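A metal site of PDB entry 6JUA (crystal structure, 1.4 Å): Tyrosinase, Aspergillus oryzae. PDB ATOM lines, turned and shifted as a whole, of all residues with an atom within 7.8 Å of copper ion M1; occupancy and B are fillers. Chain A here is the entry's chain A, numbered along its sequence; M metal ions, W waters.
Copper ion M1 is bound by water W1 (1.7 Å), NE2 of His 332 (1.9 Å), NE2 of His 336 (2.1 Å) and NE2 of His 376 (2.2 Å).
Phe 517 touches copper ion M1. Of the 18 residues printed, 4 come within 4 Å of copper ion M1. The nearest printed residue that does not touch copper ion M1 is Phe 372 (4.03 Å).
O of His 332 sits at hydrogen-bond distance from NE2 of His 375 (3.3 Å). ND1 of His 332 sits at hydrogen-bond distance from OD1 of Asn 333 (3.0 Å). O of Glu 329 sits at hydrogen-bond distance from ND1 of His 332 (3.2 Å). A ring nitrogen (ND1) of His 336 sits at hydrogen-bond distance from the backbone carbonyl oxygen (O) of Met 360 (2.8 Å).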
ATOM      1  N   HIS A  71      20.976   4.239  33.150  1.00  0.00           N
ATOM      2  CA  HIS A  71      21.305   3.480  31.958  1.00  0.00           C
ATOM      3  C   HIS A  71      21.471   1.990  32.194  1.00  0.00           C
ATOM      4  O   HIS A  71      21.026   1.181  31.366  1.00  0.00           O
ATOM      5  CB  HIS A  71      22.609   4.051  31.366  1.00  0.00           C
ATOM      6  CG  HIS A  71      22.959   3.543  30.006  1.00  0.00           C
ATOM      7  ND1 HIS A  71      23.973   2.652  29.773  1.00  0.00           N
ATOM      8  CD2 HIS A  71      22.431   3.794  28.784  1.00  0.00           C
ATOM      9  CE1 HIS A  71      24.065   2.369  28.490  1.00  0.00           C
ATOM     10  NE2 HIS A  71      23.134   3.059  27.865  1.00  0.00           N
ATOM     11  N   VAL A  97      17.268   1.432  26.240  1.00  0.00           N
ATOM     12  CA  VAL A  97      16.861   0.636  25.089  1.00  0.00           C
ATOM     13  C   VAL A  97      18.045   0.397  24.150  1.00  0.00           C
ATOM     14  O   VAL A  97      18.580   1.360  23.595  1.00  0.00           O
ATOM     15  CB  VAL A  97      15.720   1.271  24.270  1.00  0.00           C
ATOM     16  CG1 VAL A  97      15.369   0.470  23.029  1.00  0.00           C
ATOM     17  CG2 VAL A  97      14.487   1.443  25.146  1.00  0.00           C
ATOM     18  N   HIS A  98      18.358  -0.876  24.002  1.00  0.00           N
ATOM     19  CA  HIS A  98      19.344  -1.352  23.020  1.00  0.00           C
ATOM     20  C   HIS A  98      18.761  -2.440  22.140  1.00  0.00           C
ATOM     21  O   HIS A  98      17.889  -3.197  22.573  1.00  0.00           O
ATOM     22  CB  HIS A  98      20.600  -1.821  23.752  1.00  0.00           C
ATOM     23  CG  HIS A  98      21.205  -0.770  24.628  1.00  0.00           C
ATOM     24  ND1 HIS A  98      21.368  -0.956  25.988  1.00  0.00           N
ATOM     25  CD2 HIS A  98      21.675   0.475  24.370  1.00  0.00           C
ATOM     26  CE1 HIS A  98      21.929   0.118  26.513  1.00  0.00           C
ATOM     27  NE2 HIS A  98      22.127   1.011  25.561  1.00  0.00           N
ATOM     28  N   PHE A 103      15.968   2.842  20.165  1.00  0.00           N
ATOM     29  CA  PHE A 103      17.315   3.218  20.611  1.00  0.00           C
ATOM     30  C   PHE A 103      17.584   4.701  20.436  1.00  0.00           C
ATOM     31  O   PHE A 103      18.051   5.338  21.407  1.00  0.00           O
ATOM     32  CB  PHE A 103      18.372   2.354  19.916  1.00  0.00           C
ATOM     33  CG  PHE A 103      19.776   2.918  19.973  1.00  0.00           C
ATOM     34  CD1 PHE A 103      20.581   2.794  21.101  1.00  0.00           C
ATOM     35  CD2 PHE A 103      20.302   3.575  18.871  1.00  0.00           C
ATOM     36  CE1 PHE A 103      21.856   3.323  21.101  1.00  0.00           C
ATOM     37  CE2 PHE A 103      21.565   4.131  18.875  1.00  0.00           C
ATOM     38  CZ  PHE A 103      22.349   4.008  20.012  1.00  0.00           C
ATOM     39  N   HIS A 107      17.515   7.511  23.897  1.00  0.00           N
ATOM     40  CA  HIS A 107      18.760   8.229  24.186  1.00  0.00           C
ATOM     41  C   HIS A 107      18.616   9.719  23.910  1.00  0.00           C
ATOM     42  O   HIS A 107      19.284  10.535  24.572  1.00  0.00           O
ATOM     43  CB  HIS A 107      19.941   7.570  23.456  1.00  0.00           C
ATOM     44  CG  HIS A 107      20.368   6.243  24.009  1.00  0.00           C
ATOM     45  ND1 HIS A 107      19.754   5.063  23.652  1.00  0.00           N
ATOM     46  CD2 HIS A 107      21.319   5.897  24.913  1.00  0.00           C
ATOM     47  CE1 HIS A 107      20.312   4.047  24.294  1.00  0.00           C
ATOM     48  NE2 HIS A 107      21.271   4.525  25.064  1.00  0.00           N
ATOM     49  N   GLU A 329      23.144   2.434  15.335  1.00  0.00           N
ATOM     50  CA  GLU A 329      23.489   1.757  16.596  1.00  0.00           C
ATOM     51  C   GLU A 329      24.771   0.946  16.467  1.00  0.00           C
ATOM     52  O   GLU A 329      25.615   0.945  17.374  1.00  0.00           O
ATOM     53  CB  GLU A 329      22.316   0.870  17.040  1.00  0.00           C
ATOM     54  CG  GLU A 329      22.507   0.253  18.417  1.00  0.00           C
ATOM     55  CD  GLU A 329      21.283  -0.468  18.937  1.00  0.00           C
ATOM     56  OE1 GLU A 329      20.314  -0.672  18.172  1.00  0.00           O
ATOM     57  OE2 GLU A 329      21.304  -0.838  20.147  1.00  0.00           O
ATOM     58  N   HIS A 332      27.648   3.312  16.643  1.00  0.00           N
ATOM     59  CA  HIS A 332      27.714   3.697  18.057  1.00  0.00           C
ATOM     60  C   HIS A 332      28.354   2.625  18.937  1.00  0.00           C
ATOM     61  O   HIS A 332      29.057   2.939  19.904  1.00  0.00           O
ATOM     62  CB  HIS A 332      26.303   4.076  18.530  1.00  0.00           C
ATOM     63  CG  HIS A 332      25.925   3.650  19.903  1.00  0.00           C
ATOM     64  ND1 HIS A 332      25.476   2.377  20.197  1.00  0.00           N
ATOM     65  CD2 HIS A 332      25.887   4.316  21.081  1.00  0.00           C
ATOM     66  CE1 HIS A 332      25.194   2.275  21.491  1.00  0.00           C
ATOM     67  NE2 HIS A 332      25.435   3.445  22.046  1.00  0.00           N
ATOM     68  N   ASN A 333      28.135   1.360  18.607  1.00  0.00           N
ATOM     69  CA  ASN A 333      28.675   0.221  19.354  1.00  0.00           C
ATOM     70  C   ASN A 333      30.185   0.142  19.201  1.00  0.00           C
ATOM     71  O   ASN A 333      30.889  -0.087  20.185  1.00  0.00           O
ATOM     72  CB  ASN A 333      28.054  -1.096  18.872  1.00  0.00           C
ATOM     73  CG  ASN A 333      26.631  -1.332  19.323  1.00  0.00           C
ATOM     74  OD1 ASN A 333      26.048  -0.573  20.094  1.00  0.00           O
ATOM     75  ND2 ASN A 333      26.038  -2.426  18.836  1.00  0.00           N
ATOM     76  N   HIS A 336      31.887   2.870  21.326  1.00  0.00           N
ATOM     77  CA  HIS A 336      31.950   2.482  22.728  1.00  0.00           C
ATOM     78  C   HIS A 336      33.192   1.635  22.990  1.00  0.00           C
ATOM     79  O   HIS A 336      33.965   1.899  23.918  1.00  0.00           O
ATOM     80  CB  HIS A 336      30.672   1.729  23.131  1.00  0.00           C
ATOM     81  CG  HIS A 336      29.554   2.563  23.668  1.00  0.00           C
ATOM     82  ND1 HIS A 336      29.569   3.105  24.935  1.00  0.00           N
ATOM     83  CD2 HIS A 336      28.343   2.930  23.159  1.00  0.00           C
ATOM     84  CE1 HIS A 336      28.452   3.771  25.173  1.00  0.00           C
ATOM     85  NE2 HIS A 336      27.683   3.686  24.097  1.00  0.00           N
ATOM     86  N   MET A 360      33.638   2.556  29.046  1.00  0.00           N
ATOM     87  CA  MET A 360      32.810   2.822  27.852  1.00  0.00           C
ATOM     88  C   MET A 360      32.479   1.613  27.021  1.00  0.00           C
ATOM     89  O   MET A 360      31.523   1.626  26.238  1.00  0.00           O
ATOM     90  CB  MET A 360      33.513   3.913  27.025  1.00  0.00           C
ATOM     91  CG  MET A 360      33.064   5.305  27.447  1.00  0.00           C
ATOM     92  SD  MET A 360      31.395   5.723  26.920  1.00  0.00           S
ATOM     93  CE  MET A 360      31.570   6.003  25.178  1.00  0.00           C
ATOM     94  N   VAL A 363      28.097  -2.119  28.645  1.00  0.00           N
ATOM     95  CA  VAL A 363      26.761  -1.544  28.791  1.00  0.00           C
ATOM     96  C   VAL A 363      26.407  -1.206  30.233  1.00  0.00           C
ATOM     97  O   VAL A 363      25.914  -0.102  30.508  1.00  0.00           O
ATOM     98  CB  VAL A 363      25.675  -2.483  28.229  1.00  0.00           C
ATOM     99  CG1 VAL A 363      24.287  -1.927  28.499  1.00  0.00           C
ATOM    100  CG2 VAL A 363      25.905  -2.676  26.737  1.00  0.00           C
ATOM    101  N   ALA A 366      28.876   1.988  31.205  1.00  0.00           N
ATOM    102  CA  ALA A 366      29.444   2.978  30.286  1.00  0.00           C
ATOM    103  C   ALA A 366      29.013   4.406  30.617  1.00  0.00           C
ATOM    104  O   ALA A 366      29.794   5.351  30.393  1.00  0.00           O
ATOM    105  CB  ALA A 366      29.144   2.643  28.831  1.00  0.00           C
ATOM    106  N   ALA A 367      27.825   4.598  31.145  1.00  0.00           N
ATOM    107  CA  ALA A 367      27.270   5.935  31.374  1.00  0.00           C
ATOM    108  C   ALA A 367      28.034   6.708  32.436  1.00  0.00           C
ATOM    109  O   ALA A 367      27.922   7.949  32.521  1.00  0.00           O
ATOM    110  CB  ALA A 367      25.791   5.859  31.731  1.00  0.00           C
ATOM    111  N   PHE A 372      30.617   9.537  27.694  1.00  0.00           N
ATOM    112  CA  PHE A 372      29.372   8.877  27.284  1.00  0.00           C
ATOM    113  C   PHE A 372      28.380   9.881  26.713  1.00  0.00           C
ATOM    114  O   PHE A 372      27.746   9.660  25.679  1.00  0.00           O
ATOM    115  CB  PHE A 372      28.760   8.119  28.469  1.00  0.00           C
ATOM    116  CG  PHE A 372      27.394   7.531  28.203  1.00  0.00           C
ATOM    117  CD1 PHE A 372      26.226   8.275  28.348  1.00  0.00           C
ATOM    118  CD2 PHE A 372      27.264   6.223  27.788  1.00  0.00           C
ATOM    119  CE1 PHE A 372      24.987   7.730  28.102  1.00  0.00           C
ATOM    120  CE2 PHE A 372      26.020   5.644  27.554  1.00  0.00           C
ATOM    121  CZ  PHE A 372      24.863   6.408  27.701  1.00  0.00           C
ATOM    122  N   HIS A 375      29.401  11.508  23.363  1.00  0.00           N
ATOM    123  CA  HIS A 375      29.198  10.516  22.312  1.00  0.00           C
ATOM    124  C   HIS A 375      27.721  10.475  21.928  1.00  0.00           C
ATOM    125  O   HIS A 375      27.332  10.623  20.765  1.00  0.00           O
ATOM    126  CB  HIS A 375      29.645   9.140  22.834  1.00  0.00           C
ATOM    127  CG  HIS A 375      29.397   7.999  21.903  1.00  0.00           C
ATOM    128  ND1 HIS A 375      29.581   8.077  20.534  1.00  0.00           N
ATOM    129  CD2 HIS A 375      29.016   6.722  22.163  1.00  0.00           C
ATOM    130  CE1 HIS A 375      29.299   6.887  20.007  1.00  0.00           C
ATOM    131  NE2 HIS A 375      28.943   6.040  20.970  1.00  0.00           N
ATOM    132  N   HIS A 376      26.873  10.292  22.958  1.00  0.00           N
ATOM    133  CA  HIS A 376      25.443  10.286  22.668  1.00  0.00           C
ATOM    134  C   HIS A 376      24.928  11.617  22.158  1.00  0.00           C
ATOM    135  O   HIS A 376      23.921  11.639  21.423  1.00  0.00           O
ATOM    136  CB  HIS A 376      24.658   9.775  23.901  1.00  0.00           C
ATOM    137  CG  HIS A 376      24.571   8.276  23.783  1.00  0.00           C
ATOM    138  ND1 HIS A 376      23.647   7.645  22.973  1.00  0.00           N
ATOM    139  CD2 HIS A 376      25.341   7.325  24.339  1.00  0.00           C
ATOM    140  CE1 HIS A 376      23.857   6.343  23.053  1.00  0.00           C
ATOM    141  NE2 HIS A 376      24.868   6.121  23.880  1.00  0.00           N
ATOM    142  N   ILE A 379      25.474  11.084  18.586  1.00  0.00           N
ATOM    143  CA  ILE A 379      24.481  10.146  18.044  1.00  0.00           C
ATOM    144  C   ILE A 379      23.135  10.826  17.849  1.00  0.00           C
ATOM    145  O   ILE A 379      22.411  10.559  16.866  1.00  0.00           O
ATOM    146  CB  ILE A 379      24.391   8.897  18.952  1.00  0.00           C
ATOM    147  CG1 ILE A 379      25.710   8.112  19.002  1.00  0.00           C
ATOM    148  CG2 ILE A 379      23.235   7.980  18.580  1.00  0.00           C
ATOM    149  CD1 ILE A 379      26.300   7.735  17.659  1.00  0.00           C
ATOM    150  N   PHE A 517      28.028  -4.844  21.776  1.00  0.00           N
ATOM    151  CA  PHE A 517      27.808  -3.999  22.949  1.00  0.00           C
ATOM    152  C   PHE A 517      26.667  -4.589  23.783  1.00  0.00           C
ATOM    153  O   PHE A 517      25.506  -4.231  23.593  1.00  0.00           O
ATOM    154  CB  PHE A 517      27.552  -2.558  22.533  1.00  0.00           C
ATOM    155  CG  PHE A 517      27.501  -1.516  23.629  1.00  0.00           C
ATOM    156  CD1 PHE A 517      28.538  -1.304  24.524  1.00  0.00           C
ATOM    157  CD2 PHE A 517      26.360  -0.725  23.780  1.00  0.00           C
ATOM    158  CE1 PHE A 517      28.441  -0.364  25.531  1.00  0.00           C
ATOM    159  CE2 PHE A 517      26.252   0.233  24.751  1.00  0.00           C
ATOM    160  CZ  PHE A 517      27.305   0.431  25.639  1.00  0.00           C
HETATM  161 CU    CU M   1      25.661   4.016  23.889  1.00  0.00          CU
HETATM  162 CU    CU M   2      22.724   3.054  25.895  1.00  0.00          CU
HETATM  163  O   HOH W   1      24.761   3.463  25.236  1.00  0.00           O
